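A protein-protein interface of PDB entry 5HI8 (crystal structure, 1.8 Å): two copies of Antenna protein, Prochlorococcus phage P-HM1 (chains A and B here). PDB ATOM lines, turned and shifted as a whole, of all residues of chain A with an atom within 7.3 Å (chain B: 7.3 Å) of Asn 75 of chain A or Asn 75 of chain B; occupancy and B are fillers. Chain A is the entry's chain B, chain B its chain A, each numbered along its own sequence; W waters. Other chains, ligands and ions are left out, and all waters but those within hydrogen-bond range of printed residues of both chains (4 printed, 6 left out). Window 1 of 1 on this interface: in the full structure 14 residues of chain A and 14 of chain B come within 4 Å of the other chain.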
ATOM      1  N   LYS A  42      -9.236 -37.396  -3.946  1.00  0.00           N
ATOM      2  CA  LYS A  42     -10.216 -36.319  -4.076  1.00  0.00           C
ATOM      3  C   LYS A  42     -11.341 -36.705  -5.049  1.00  0.00           C
ATOM      4  O   LYS A  42     -11.083 -36.982  -6.200  1.00  0.00           O
ATOM      5  CB  LYS A  42      -9.544 -35.026  -4.553  1.00  0.00           C
ATOM      6  CG  LYS A  42     -10.387 -33.788  -4.297  1.00  0.00           C
ATOM      7  CD  LYS A  42      -9.994 -32.610  -5.171  1.00  0.00           C
ATOM      8  CE  LYS A  42      -8.706 -31.973  -4.754  1.00  0.00           C
ATOM      9  NZ  LYS A  42      -8.549 -30.630  -5.406  1.00  0.00           N
ATOM     10  N   THR A  45     -18.737 -36.217  -5.529  1.00  0.00           N
ATOM     11  CA  THR A  45     -19.805 -37.172  -5.282  1.00  0.00           C
ATOM     12  C   THR A  45     -21.169 -36.558  -5.612  1.00  0.00           C
ATOM     13  O   THR A  45     -21.404 -35.368  -5.402  1.00  0.00           O
ATOM     14  CB  THR A  45     -19.814 -37.669  -3.834  1.00  0.00           C
ATOM     15  OG1 THR A  45     -20.165 -36.607  -2.943  1.00  0.00           O
ATOM     16  CG2 THR A  45     -18.430 -38.240  -3.428  1.00  0.00           C
ATOM     17  N   GLU A  58     -24.965 -33.216  -3.881  1.00  0.00           N
ATOM     18  CA  GLU A  58     -23.733 -32.985  -4.621  1.00  0.00           C
ATOM     19  C   GLU A  58     -22.638 -32.331  -3.768  1.00  0.00           C
ATOM     20  O   GLU A  58     -22.884 -31.307  -3.151  1.00  0.00           O
ATOM     21  CB  GLU A  58     -24.064 -32.097  -5.826  1.00  0.00           C
ATOM     22  CG  GLU A  58     -22.998 -32.078  -6.842  1.00  0.00           C
ATOM     23  CD  GLU A  58     -23.363 -31.303  -8.080  1.00  0.00           C
ATOM     24  OE1 GLU A  58     -24.331 -30.513  -8.045  1.00  0.00           O
ATOM     25  OE2 GLU A  58     -22.662 -31.486  -9.096  1.00  0.00           O
ATOM     26  N   GLN A  59     -21.436 -32.906  -3.742  1.00  0.00           N
ATOM     27  CA  GLN A  59     -20.330 -32.287  -2.994  1.00  0.00           C
ATOM     28  C   GLN A  59     -18.982 -32.891  -3.357  1.00  0.00           C
ATOM     29  O   GLN A  59     -18.914 -33.913  -4.014  1.00  0.00           O
ATOM     30  CB  GLN A  59     -20.561 -32.413  -1.478  1.00  0.00           C
ATOM     31  CG  GLN A  59     -20.422 -33.829  -0.928  1.00  0.00           C
ATOM     32  CD  GLN A  59     -20.574 -33.897   0.584  1.00  0.00           C
ATOM     33  OE1 GLN A  59     -20.914 -32.916   1.233  1.00  0.00           O
ATOM     34  NE2 GLN A  59     -20.345 -35.070   1.141  1.00  0.00           N
ATOM     35  N   THR A  60     -17.901 -32.263  -2.901  1.00  0.00           N
ATOM     36  CA  THR A  60     -16.570 -32.772  -3.174  1.00  0.00           C
ATOM     37  C   THR A  60     -15.989 -33.254  -1.839  1.00  0.00           C
ATOM     38  O   THR A  60     -16.229 -32.642  -0.796  1.00  0.00           O
ATOM     39  CB  THR A  60     -15.682 -31.697  -3.840  1.00  0.00           C
ATOM     40  OG1 THR A  60     -16.307 -31.250  -5.054  1.00  0.00           O
ATOM     41  CG2 THR A  60     -14.329 -32.236  -4.195  1.00  0.00           C
ATOM     42  N   VAL A  61     -15.292 -34.382  -1.874  1.00  0.00           N
ATOM     43  CA  VAL A  61     -14.760 -34.975  -0.654  1.00  0.00           C
ATOM     44  C   VAL A  61     -13.261 -35.229  -0.773  1.00  0.00           C
ATOM     45  O   VAL A  61     -12.733 -35.508  -1.855  1.00  0.00           O
ATOM     46  CB  VAL A  61     -15.464 -36.324  -0.279  1.00  0.00           C
ATOM     47  CG1 VAL A  61     -16.948 -36.100  -0.016  1.00  0.00           C
ATOM     48  CG2 VAL A  61     -15.254 -37.381  -1.356  1.00  0.00           C
ATOM     49  N   ASP A  62     -12.575 -35.100   0.362  1.00  0.00           N
ATOM     50  CA  ASP A  62     -11.198 -35.522   0.492  1.00  0.00           C
ATOM     51  C   ASP A  62     -11.189 -36.893   1.163  1.00  0.00           C
ATOM     52  O   ASP A  62     -11.901 -37.092   2.139  1.00  0.00           O
ATOM     53  CB  ASP A  62     -10.385 -34.540   1.345  1.00  0.00           C
ATOM     54  CG  ASP A  62     -10.126 -33.221   0.660  1.00  0.00           C
ATOM     55  OD1 ASP A  62      -9.859 -33.199  -0.560  1.00  0.00           O
ATOM     56  OD2 ASP A  62     -10.167 -32.197   1.364  1.00  0.00           O
ATOM     57  N   GLU A  64      -9.120 -39.246   3.491  1.00  0.00           N
ATOM     58  CA  GLU A  64      -8.046 -39.137   4.483  1.00  0.00           C
ATOM     59  C   GLU A  64      -7.836 -40.482   5.167  1.00  0.00           C
ATOM     60  O   GLU A  64      -8.777 -41.238   5.386  1.00  0.00           O
ATOM     61  CB  GLU A  64      -8.385 -38.069   5.527  1.00  0.00           C
ATOM     62  CG  GLU A  64      -8.883 -36.738   4.929  1.00  0.00           C
ATOM     63  CD  GLU A  64      -9.489 -35.779   5.960  1.00  0.00           C
ATOM     64  OE1 GLU A  64      -9.463 -34.551   5.710  1.00  0.00           O
ATOM     65  OE2 GLU A  64     -10.011 -36.241   7.000  1.00  0.00           O
ATOM     66  N   ILE A  72     -11.453 -41.725   6.398  1.00  0.00           N
ATOM     67  CA  ILE A  72     -12.428 -40.640   6.520  1.00  0.00           C
ATOM     68  C   ILE A  72     -12.778 -40.088   5.136  1.00  0.00           C
ATOM     69  O   ILE A  72     -11.894 -39.674   4.393  1.00  0.00           O
ATOM     70  CB  ILE A  72     -11.888 -39.502   7.428  1.00  0.00           C
ATOM     71  CG1 ILE A  72     -11.553 -40.049   8.821  1.00  0.00           C
ATOM     72  CG2 ILE A  72     -12.906 -38.341   7.508  1.00  0.00           C
ATOM     73  CD1 ILE A  72     -10.994 -39.018   9.784  1.00  0.00           C
ATOM     74  N   VAL A  73     -14.068 -40.101   4.791  1.00  0.00           N
ATOM     75  CA  VAL A  73     -14.543 -39.378   3.617  1.00  0.00           C
ATOM     76  C   VAL A  73     -14.967 -38.019   4.129  1.00  0.00           C
ATOM     77  O   VAL A  73     -16.020 -37.879   4.753  1.00  0.00           O
ATOM     78  CB  VAL A  73     -15.705 -40.100   2.888  1.00  0.00           C
ATOM     79  CG1 VAL A  73     -16.166 -39.287   1.653  1.00  0.00           C
ATOM     80  CG2 VAL A  73     -15.270 -41.504   2.470  1.00  0.00           C
ATOM     81  N   HIS A  74     -14.123 -37.029   3.866  1.00  0.00           N
ATOM     82  CA  HIS A  74     -14.236 -35.731   4.505  1.00  0.00           C
ATOM     83  C   HIS A  74     -14.956 -34.673   3.690  1.00  0.00           C
ATOM     84  O   HIS A  74     -14.629 -34.439   2.541  1.00  0.00           O
ATOM     85  CB  HIS A  74     -12.853 -35.188   4.839  1.00  0.00           C
ATOM     86  CG  HIS A  74     -12.829 -33.719   5.088  1.00  0.00           C
ATOM     87  ND1 HIS A  74     -13.452 -33.132   6.169  1.00  0.00           N
ATOM     88  CD2 HIS A  74     -12.268 -32.709   4.385  1.00  0.00           C
ATOM     89  CE1 HIS A  74     -13.283 -31.825   6.117  1.00  0.00           C
ATOM     90  NE2 HIS A  74     -12.560 -31.542   5.048  1.00  0.00           N
ATOM     91  N   ASN A  75     -15.884 -34.013   4.356  1.00  0.00           N
ATOM     92  CA  ASN A  75     -16.448 -32.749   3.904  1.00  0.00           C
ATOM     93  C   ASN A  75     -16.806 -31.955   5.144  1.00  0.00           C
ATOM     94  O   ASN A  75     -17.233 -32.534   6.138  1.00  0.00           O
ATOM     95  CB  ASN A  75     -17.667 -32.986   3.023  1.00  0.00           C
ATOM     96  CG  ASN A  75     -18.198 -31.700   2.429  1.00  0.00           C
ATOM     97  OD1 ASN A  75     -18.865 -30.931   3.104  1.00  0.00           O
ATOM     98  ND2 ASN A  75     -17.856 -31.448   1.170  1.00  0.00           N
ATOM     99  N   PRO A  76     -16.629 -30.626   5.114  1.00  0.00           N
ATOM    100  CA  PRO A  76     -16.923 -29.896   6.342  1.00  0.00           C
ATOM    101  C   PRO A  76     -18.353 -30.048   6.835  1.00  0.00           C
ATOM    102  O   PRO A  76     -18.581 -29.876   8.034  1.00  0.00           O
ATOM    103  CB  PRO A  76     -16.620 -28.442   5.964  1.00  0.00           C
ATOM    104  CG  PRO A  76     -15.631 -28.541   4.881  1.00  0.00           C
ATOM    105  CD  PRO A  76     -15.965 -29.772   4.114  1.00  0.00           C
ATOM    106  N   ALA A  77     -19.295 -30.369   5.946  1.00  0.00           N
ATOM    107  CA  ALA A  77     -20.667 -30.572   6.370  1.00  0.00           C
ATOM    108  C   ALA A  77     -20.806 -31.826   7.218  1.00  0.00           C
ATOM    109  O   ALA A  77     -21.551 -31.838   8.206  1.00  0.00           O
ATOM    110  CB  ALA A  77     -21.599 -30.650   5.140  1.00  0.00           C
ATOM    111  N   CYS A  78     -20.081 -32.878   6.841  1.00  0.00           N
ATOM    112  CA  CYS A  78     -20.272 -34.189   7.462  1.00  0.00           C
ATOM    113  C   CYS A  78     -19.202 -35.183   7.019  1.00  0.00           C
ATOM    114  O   CYS A  78     -19.171 -35.617   5.863  1.00  0.00           O
ATOM    115  CB  CYS A  78     -21.672 -34.736   7.119  1.00  0.00           C
ATOM    116  SG  CYS A  78     -22.020 -36.395   7.805  1.00  0.00           S
ATOM    117  N   ASP A  79     -18.320 -35.529   7.946  1.00  0.00           N
ATOM    118  CA  ASP A  79     -17.347 -36.592   7.728  1.00  0.00           C
ATOM    119  C   ASP A  79     -17.999 -37.949   7.912  1.00  0.00           C
ATOM    120  O   ASP A  79     -18.764 -38.153   8.857  1.00  0.00           O
ATOM    121  CB  ASP A  79     -16.172 -36.494   8.710  1.00  0.00           C
ATOM    122  CG  ASP A  79     -15.243 -35.343   8.427  1.00  0.00           C
ATOM    123  OD1 ASP A  79     -15.317 -34.721   7.346  1.00  0.00           O
ATOM    124  OD2 ASP A  79     -14.398 -35.070   9.310  1.00  0.00           O
ATOM    125  N   ILE A  80     -17.678 -38.883   7.026  1.00  0.00           N
ATOM    126  CA  ILE A  80     -18.105 -40.264   7.198  1.00  0.00           C
ATOM    127  C   ILE A  80     -16.860 -41.064   7.515  1.00  0.00           C
ATOM    128  O   ILE A  80     -15.910 -41.045   6.737  1.00  0.00           O
ATOM    129  CB  ILE A  80     -18.780 -40.863   5.954  1.00  0.00           C
ATOM    130  CG1 ILE A  80     -19.955 -39.995   5.472  1.00  0.00           C
ATOM    131  CG2 ILE A  80     -19.242 -42.278   6.261  1.00  0.00           C
ATOM    132  CD1 ILE A  80     -20.907 -39.598   6.553  1.00  0.00           C
ATOM    133  N   GLU A  94     -19.890 -38.632  11.499  1.00  0.00           N
ATOM    134  CA  GLU A  94     -19.483 -37.967  12.720  1.00  0.00           C
ATOM    135  C   GLU A  94     -20.724 -37.438  13.435  1.00  0.00           C
ATOM    136  O   GLU A  94     -21.765 -37.228  12.800  1.00  0.00           O
ATOM    137  CB  GLU A  94     -18.509 -36.828  12.418  1.00  0.00           C
ATOM    138  CG  GLU A  94     -19.099 -35.692  11.570  1.00  0.00           C
ATOM    139  CD  GLU A  94     -18.135 -34.525  11.397  1.00  0.00           C
ATOM    140  OE1 GLU A  94     -18.063 -33.957  10.284  1.00  0.00           O
ATOM    141  OE2 GLU A  94     -17.447 -34.175  12.380  1.00  0.00           O
ATOM    142  N   GLN A  98     -24.445 -32.591   9.483  1.00  0.00           N
ATOM    143  CA  GLN A  98     -25.607 -31.833   9.027  1.00  0.00           C
ATOM    144  C   GLN A  98     -25.592 -31.686   7.507  1.00  0.00           C
ATOM    145  O   GLN A  98     -24.534 -31.535   6.907  1.00  0.00           O
ATOM    146  CB  GLN A  98     -25.636 -30.444   9.652  1.00  0.00           C
ATOM    147  CG  GLN A  98     -25.537 -30.425  11.153  1.00  0.00           C
ATOM    148  CD  GLN A  98     -24.818 -29.199  11.647  1.00  0.00           C
ATOM    149  OE1 GLN A  98     -25.364 -28.094  11.617  1.00  0.00           O
ATOM    150  NE2 GLN A  98     -23.570 -29.379  12.092  1.00  0.00           N
ATOM    151  N   LYS B  42     -17.141 -22.809  11.646  1.00  0.00           N
ATOM    152  CA  LYS B  42     -17.858 -23.634  10.681  1.00  0.00           C
ATOM    153  C   LYS B  42     -19.104 -22.915  10.135  1.00  0.00           C
ATOM    154  O   LYS B  42     -19.993 -22.574  10.890  1.00  0.00           O
ATOM    155  CB  LYS B  42     -18.276 -24.965  11.309  1.00  0.00           C
ATOM    156  CG  LYS B  42     -18.630 -26.021  10.277  1.00  0.00           C
ATOM    157  CD  LYS B  42     -19.481 -27.150  10.846  1.00  0.00           C
ATOM    158  CE  LYS B  42     -18.729 -28.052  11.771  1.00  0.00           C
ATOM    159  NZ  LYS B  42     -19.496 -29.323  12.012  1.00  0.00           N
ATOM    160  N   THR B  45     -22.580 -21.888   3.641  1.00  0.00           N
ATOM    161  CA  THR B  45     -22.593 -20.769   2.710  1.00  0.00           C
ATOM    162  C   THR B  45     -23.551 -21.053   1.550  1.00  0.00           C
ATOM    163  O   THR B  45     -23.678 -22.188   1.091  1.00  0.00           O
ATOM    164  CB  THR B  45     -21.207 -20.468   2.153  1.00  0.00           C
ATOM    165  OG1 THR B  45     -20.750 -21.554   1.347  1.00  0.00           O
ATOM    166  CG2 THR B  45     -20.201 -20.204   3.299  1.00  0.00           C
ATOM    167  N   GLU B  58     -24.197 -23.791  -3.007  1.00  0.00           N
ATOM    168  CA  GLU B  58     -24.403 -24.156  -1.614  1.00  0.00           C
ATOM    169  C   GLU B  58     -23.331 -25.105  -1.093  1.00  0.00           C
ATOM    170  O   GLU B  58     -23.084 -26.125  -1.712  1.00  0.00           O
ATOM    171  CB  GLU B  58     -25.777 -24.810  -1.499  1.00  0.00           C
ATOM    172  CG  GLU B  58     -26.264 -24.905  -0.117  1.00  0.00           C
ATOM    173  CD  GLU B  58     -27.668 -25.441  -0.015  1.00  0.00           C
ATOM    174  OE1 GLU B  58     -28.172 -26.014  -1.002  1.00  0.00           O
ATOM    175  OE2 GLU B  58     -28.264 -25.285   1.071  1.00  0.00           O
ATOM    176  N   GLN B  59     -22.719 -24.787   0.051  1.00  0.00           N
ATOM    177  CA  GLN B  59     -21.730 -25.697   0.636  1.00  0.00           C
ATOM    178  C   GLN B  59     -21.391 -25.336   2.078  1.00  0.00           C
ATOM    179  O   GLN B  59     -21.739 -24.276   2.558  1.00  0.00           O
ATOM    180  CB  GLN B  59     -20.452 -25.709  -0.218  1.00  0.00           C
ATOM    181  CG  GLN B  59     -19.605 -24.448  -0.118  1.00  0.00           C
ATOM    182  CD  GLN B  59     -18.307 -24.547  -0.902  1.00  0.00           C
ATOM    183  OE1 GLN B  59     -18.050 -25.533  -1.594  1.00  0.00           O
ATOM    184  NE2 GLN B  59     -17.494 -23.512  -0.810  1.00  0.00           N
ATOM    185  N   THR B  60     -20.669 -26.216   2.772  1.00  0.00           N
ATOM    186  CA  THR B  60     -20.282 -25.942   4.148  1.00  0.00           C
ATOM    187  C   THR B  60     -18.761 -25.768   4.174  1.00  0.00           C
ATOM    188  O   THR B  60     -18.042 -26.451   3.440  1.00  0.00           O
ATOM    189  CB  THR B  60     -20.750 -27.073   5.093  1.00  0.00           C
ATOM    190  OG1 THR B  60     -22.179 -27.205   4.991  1.00  0.00           O
ATOM    191  CG2 THR B  60     -20.402 -26.785   6.523  1.00  0.00           C
ATOM    192  N   VAL B  61     -18.301 -24.801   4.950  1.00  0.00           N
ATOM    193  CA  VAL B  61     -16.874 -24.473   4.980  1.00  0.00           C
ATOM    194  C   VAL B  61     -16.344 -24.508   6.403  1.00  0.00           C
ATOM    195  O   VAL B  61     -17.052 -24.191   7.363  1.00  0.00           O
ATOM    196  CB  VAL B  61     -16.559 -23.071   4.359  1.00  0.00           C
ATOM    197  CG1 VAL B  61     -16.968 -23.027   2.884  1.00  0.00           C
ATOM    198  CG2 VAL B  61     -17.242 -21.943   5.129  1.00  0.00           C
ATOM    199  N   ASP B  62     -15.080 -24.919   6.521  1.00  0.00           N
ATOM    200  CA  ASP B  62     -14.321 -24.777   7.745  1.00  0.00           C
ATOM    201  C   ASP B  62     -13.443 -23.534   7.631  1.00  0.00           C
ATOM    202  O   ASP B  62     -12.834 -23.310   6.589  1.00  0.00           O
ATOM    203  CB  ASP B  62     -13.428 -25.999   7.988  1.00  0.00           C
ATOM    204  CG  ASP B  62     -14.213 -27.258   8.322  1.00  0.00           C
ATOM    205  OD1 ASP B  62     -15.224 -27.180   9.051  1.00  0.00           O
ATOM    206  OD2 ASP B  62     -13.801 -28.327   7.864  1.00  0.00           O
ATOM    207  N   GLU B  64     -10.070 -21.952   8.773  1.00  0.00           N
ATOM    208  CA  GLU B  64      -8.777 -22.385   9.300  1.00  0.00           C
ATOM    209  C   GLU B  64      -7.830 -21.198   9.362  1.00  0.00           C
ATOM    210  O   GLU B  64      -7.880 -20.304   8.517  1.00  0.00           O
ATOM    211  CB  GLU B  64      -8.186 -23.489   8.416  1.00  0.00           C
ATOM    212  CG  GLU B  64      -9.168 -24.623   8.079  1.00  0.00           C
ATOM    213  CD  GLU B  64      -8.682 -25.557   6.969  1.00  0.00           C
ATOM    214  OE1 GLU B  64      -9.129 -26.726   6.948  1.00  0.00           O
ATOM    215  OE2 GLU B  64      -7.879 -25.136   6.108  1.00  0.00           O
ATOM    216  N   ILE B  72      -7.909 -19.447   5.752  1.00  0.00           N
ATOM    217  CA  ILE B  72      -8.412 -20.325   4.697  1.00  0.00           C
ATOM    218  C   ILE B  72      -9.901 -20.623   4.912  1.00  0.00           C
ATOM    219  O   ILE B  72     -10.292 -21.124   5.967  1.00  0.00           O
ATOM    220  CB  ILE B  72      -7.608 -21.647   4.651  1.00  0.00           C
ATOM    221  CG1 ILE B  72      -6.110 -21.343   4.458  1.00  0.00           C
ATOM    222  CG2 ILE B  72      -8.157 -22.570   3.558  1.00  0.00           C
ATOM    223  CD1 ILE B  72      -5.222 -22.570   4.395  1.00  0.00           C
ATOM    224  N   VAL B  73     -10.728 -20.313   3.908  1.00  0.00           N
ATOM    225  CA  VAL B  73     -12.111 -20.772   3.895  1.00  0.00           C
ATOM    226  C   VAL B  73     -12.096 -22.075   3.122  1.00  0.00           C
ATOM    227  O   VAL B  73     -11.986 -22.082   1.894  1.00  0.00           O
ATOM    228  CB  VAL B  73     -13.089 -19.747   3.251  1.00  0.00           C
ATOM    229  CG1 VAL B  73     -14.535 -20.283   3.257  1.00  0.00           C
ATOM    230  CG2 VAL B  73     -13.018 -18.409   3.983  1.00  0.00           C
ATOM    231  N   HIS B  74     -12.184 -23.170   3.867  1.00  0.00           N
ATOM    232  CA  HIS B  74     -11.889 -24.488   3.338  1.00  0.00           C
ATOM    233  C   HIS B  74     -13.114 -25.274   2.900  1.00  0.00           C
ATOM    234  O   HIS B  74     -14.067 -25.415   3.644  1.00  0.00           O
ATOM    235  CB  HIS B  74     -11.139 -25.322   4.373  1.00  0.00           C
ATOM    236  CG  HIS B  74     -11.197 -26.790   4.105  1.00  0.00           C
ATOM    237  ND1 HIS B  74     -10.611 -27.365   3.001  1.00  0.00           N
ATOM    238  CD2 HIS B  74     -11.801 -27.792   4.781  1.00  0.00           C
ATOM    239  CE1 HIS B  74     -10.847 -28.666   3.009  1.00  0.00           C
ATOM    240  NE2 HIS B  74     -11.562 -28.950   4.080  1.00  0.00           N
ATOM    241  N   ASN B  75     -13.020 -25.811   1.699  1.00  0.00           N
ATOM    242  CA  ASN B  75     -13.889 -26.877   1.237  1.00  0.00           C
ATOM    243  C   ASN B  75     -13.075 -27.737   0.285  1.00  0.00           C
ATOM    244  O   ASN B  75     -12.250 -27.218  -0.452  1.00  0.00           O
ATOM    245  CB  ASN B  75     -15.128 -26.303   0.549  1.00  0.00           C
ATOM    246  CG  ASN B  75     -16.116 -27.364   0.162  1.00  0.00           C
ATOM    247  OD1 ASN B  75     -15.944 -28.039  -0.848  1.00  0.00           O
ATOM    248  ND2 ASN B  75     -17.148 -27.531   0.975  1.00  0.00           N
ATOM    249  N   PRO B  76     -13.299 -29.055   0.285  1.00  0.00           N
ATOM    250  CA  PRO B  76     -12.461 -29.878  -0.590  1.00  0.00           C
ATOM    251  C   PRO B  76     -12.555 -29.497  -2.066  1.00  0.00           C
ATOM    252  O   PRO B  76     -11.601 -29.745  -2.806  1.00  0.00           O
ATOM    253  CB  PRO B  76     -12.988 -31.292  -0.342  1.00  0.00           C
ATOM    254  CG  PRO B  76     -13.526 -31.258   1.021  1.00  0.00           C
ATOM    255  CD  PRO B  76     -14.110 -29.881   1.195  1.00  0.00           C
ATOM    256  N   ALA B  77     -13.672 -28.897  -2.488  1.00  0.00           N
ATOM    257  CA  ALA B  77     -13.799 -28.472  -3.874  1.00  0.00           C
ATOM    258  C   ALA B  77     -12.854 -27.333  -4.203  1.00  0.00           C
ATOM    259  O   ALA B  77     -12.251 -27.291  -5.286  1.00  0.00           O
ATOM    260  CB  ALA B  77     -15.256 -28.055  -4.178  1.00  0.00           C
ATOM    261  N   CYS B  78     -12.712 -26.404  -3.265  1.00  0.00           N
ATOM    262  CA  CYS B  78     -11.964 -25.181  -3.533  1.00  0.00           C
ATOM    263  C   CYS B  78     -11.738 -24.380  -2.263  1.00  0.00           C
ATOM    264  O   CYS B  78     -12.681 -23.832  -1.681  1.00  0.00           O
ATOM    265  CB  CYS B  78     -12.723 -24.328  -4.568  1.00  0.00           C
ATOM    266  SG  CYS B  78     -11.940 -22.741  -4.957  1.00  0.00           S
ATOM    267  N   ASP B  79     -10.488 -24.324  -1.827  1.00  0.00           N
ATOM    268  CA  ASP B  79     -10.093 -23.444  -0.740  1.00  0.00           C
ATOM    269  C   ASP B  79      -9.923 -22.025  -1.239  1.00  0.00           C
ATOM    270  O   ASP B  79      -9.351 -21.811  -2.306  1.00  0.00           O
ATOM    271  CB  ASP B  79      -8.754 -23.889  -0.108  1.00  0.00           C
ATOM    272  CG  ASP B  79      -8.868 -25.153   0.701  1.00  0.00           C
ATOM    273  OD1 ASP B  79      -9.994 -25.602   0.993  1.00  0.00           O
ATOM    274  OD2 ASP B  79      -7.800 -25.698   1.064  1.00  0.00           O
ATOM    275  N   ILE B  80     -10.404 -21.062  -0.459  1.00  0.00           N
ATOM    276  CA  ILE B  80     -10.134 -19.652  -0.722  1.00  0.00           C
ATOM    277  C   ILE B  80      -9.196 -19.166   0.359  1.00  0.00           C
ATOM    278  O   ILE B  80      -9.501 -19.298   1.546  1.00  0.00           O
ATOM    279  CB  ILE B  80     -11.403 -18.777  -0.713  1.00  0.00           C
ATOM    280  CG1 ILE B  80     -12.468 -19.329  -1.661  1.00  0.00           C
ATOM    281  CG2 ILE B  80     -11.051 -17.336  -1.075  1.00  0.00           C
ATOM    282  CD1 ILE B  80     -11.955 -19.638  -3.042  1.00  0.00           C
ATOM    283  N   GLU B  94      -7.323 -21.442  -4.357  1.00  0.00           N
ATOM    284  CA  GLU B  94      -6.199 -22.317  -4.600  1.00  0.00           C
ATOM    285  C   GLU B  94      -6.163 -22.674  -6.083  1.00  0.00           C
ATOM    286  O   GLU B  94      -7.181 -22.587  -6.765  1.00  0.00           O
ATOM    287  CB  GLU B  94      -6.296 -23.583  -3.741  1.00  0.00           C
ATOM    288  CG  GLU B  94      -7.523 -24.460  -4.033  1.00  0.00           C
ATOM    289  CD  GLU B  94      -7.525 -25.754  -3.240  1.00  0.00           C
ATOM    290  OE1 GLU B  94      -8.607 -26.165  -2.770  1.00  0.00           O
ATOM    291  OE2 GLU B  94      -6.440 -26.363  -3.089  1.00  0.00           O
ATOM    292  N   GLN B  98     -12.126 -26.169  -8.332  1.00  0.00           N
ATOM    293  CA  GLN B  98     -13.152 -26.620  -9.272  1.00  0.00           C
ATOM    294  C   GLN B  98     -14.533 -26.575  -8.628  1.00  0.00           C
ATOM    295  O   GLN B  98     -14.674 -26.858  -7.442  1.00  0.00           O
ATOM    296  CB  GLN B  98     -12.878 -28.040  -9.743  1.00  0.00           C
ATOM    297  CG  GLN B  98     -11.497 -28.266 -10.294  1.00  0.00           C
ATOM    298  CD  GLN B  98     -11.011 -29.659 -10.016  1.00  0.00           C
ATOM    299  OE1 GLN B  98     -11.477 -30.624 -10.631  1.00  0.00           O
ATOM    300  NE2 GLN B  98     -10.081 -29.788  -9.064  1.00  0.00           N
HETATM  301  O   HOH W   1     -23.569 -28.216   7.113  1.00  0.00           O
HETATM  302  O   HOH W   2     -17.983 -29.746  -1.430  1.00  0.00           O
HETATM  303  O   HOH W   3     -14.899 -30.294  -7.084  1.00  0.00           O
HETATM  304  O   HOH W   4     -19.891 -28.807   1.710  1.00  0.00           O
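A ring nitrogen (NE2) of His 74 of chain A is in hydrogen-bond range of a ring nitrogen (NE2) of His 74 of chain B, at 2.9 Å.
Among the printed residues, merely in contact across the chains: Thr 60 of chain A with Pro 76 of chain B (3.5 Å), Thr 60 of chain A with Ala 77 of chain B (3.5 Å), Val 61 of chain A with Pro 76 of chain B (3.97 Å), Asp 62 of chain A with His 74 of chain B (3.95 Å), Asp 62 of chain A with Pro 76 of chain B (3.4 Å), His 74 of chain A with Asp 62 of chain B (3.9 Å), His 74 of chain A with Pro 76 of chain B (3.7 Å), Asn 75 of chain A with Asn 75 of chain B (3.99 Å), Pro 76 of chain A with Thr 60 of chain B (3.5 Å), Pro 76 of chain A with Val 61 of chain B (3.97 Å), Pro 76 of chain A with Asp 62 of chain B (3.4 Å), Pro 76 of chain A with His 74 of chain B (3.7 Å), Pro 76 of chain A with Pro 76 of chain B (3.5 Å) and Ala 77 of chain A with Thr 60 of chain B (3.5 Å).
Thr 60 of chain A touches Ala 77 of chain B, and with the chains exchanged Ala 77 of chain A touches Thr 60 of chain B.
Val 61 of chain A touches Pro 76 of chain B, and with the chains exchanged Pro 76 of chain A touches Val 61 of chain B.
His 74 of chain A touches Pro 76 of chain B, and with the chains exchanged Pro 76 of chain A touches His 74 of chain B.
19 positions are printed for both chains.
Printed residues of chain B that touch a printed residue of chain A: Thr 60, Val 61, Asp 62, His 74, Asn 75, Pro 76 and Ala 77.
Hydrophobic or aromatic side chains of chain B that line the printed part of chain A: His 74, Pro 76 and Ala 77.
Of the 19 printed residues of chain A, 7 touch a printed residue of chain B.
Printed residues of chain A that touch a printed residue of chain B: Thr 60, Val 61, Asp 62, His 74, Asn 75, Pro 76 and Ala 77.
Among the printed residues, 15 pairs touch across the chains.
Among the printed residues, no Asp or Glu carboxylate lies within 4 Å of a Lys or Arg side-chain nitrogen of the other chain.
Water W3 bridges the side-chain hydroxyl (OG1) of Thr 60 of chain A and the backbone carbonyl oxygen (O) of Gln 98 of chain B.
Water W1 lies within hydrogen-bond range of OG1 of Thr 60 of chain B and O of Gln 98 of chain A.
Water W4 lies within hydrogen-bond range of the side-chain amide oxygen of Asn 75 of chain A (2.7 Å), the backbone NH of Thr 60 of chain B (2.9 Å) and the side-chain amide nitrogen of Asn 75 of chain B (3.1 Å).
Printed residues of chain B within 4 Å of Asn 75 of chain A: Asn 75 (3.99 Å).
Of the printed residues of chain B, Ala 77 of chain A touches Thr 60 (3.5 Å).
Ile 80 of chain A touches none of the printed residues of chain B.
Of the printed residues of chain A, Val 61 of chain B touches Pro 76.
Glu 64 of chain B touches none of the printed residues of chain A.
Of the printed residues of chain A, Asn 75 of chain B touches Asn 75 (3.99 Å).
The nearest printed residue of chain B that does not touch Asn 75 of chain A is Pro 76 of chain B (4.1 Å).
The nearest printed residue of chain B that does not touch Thr 60 of chain A is Asn 75 of chain B (4.6 Å).
The backbone NH of His 74 of chain B sits at hydrogen-bond distance from the backbone carbonyl oxygen of Asp 62 of chain B, at 2.8 Å.
ND1 of His 74 of chain B lies within hydrogen-bond range of OD1 of Asp 79 of chain B.
OD1 of Asn 75 of chain B sits close to OE1 of Gln 59 of chain B, at 3.4 Å.
O of Thr 60 of chain B sits at hydrogen-bond distance from ND2 of Asn 75 of chain B.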
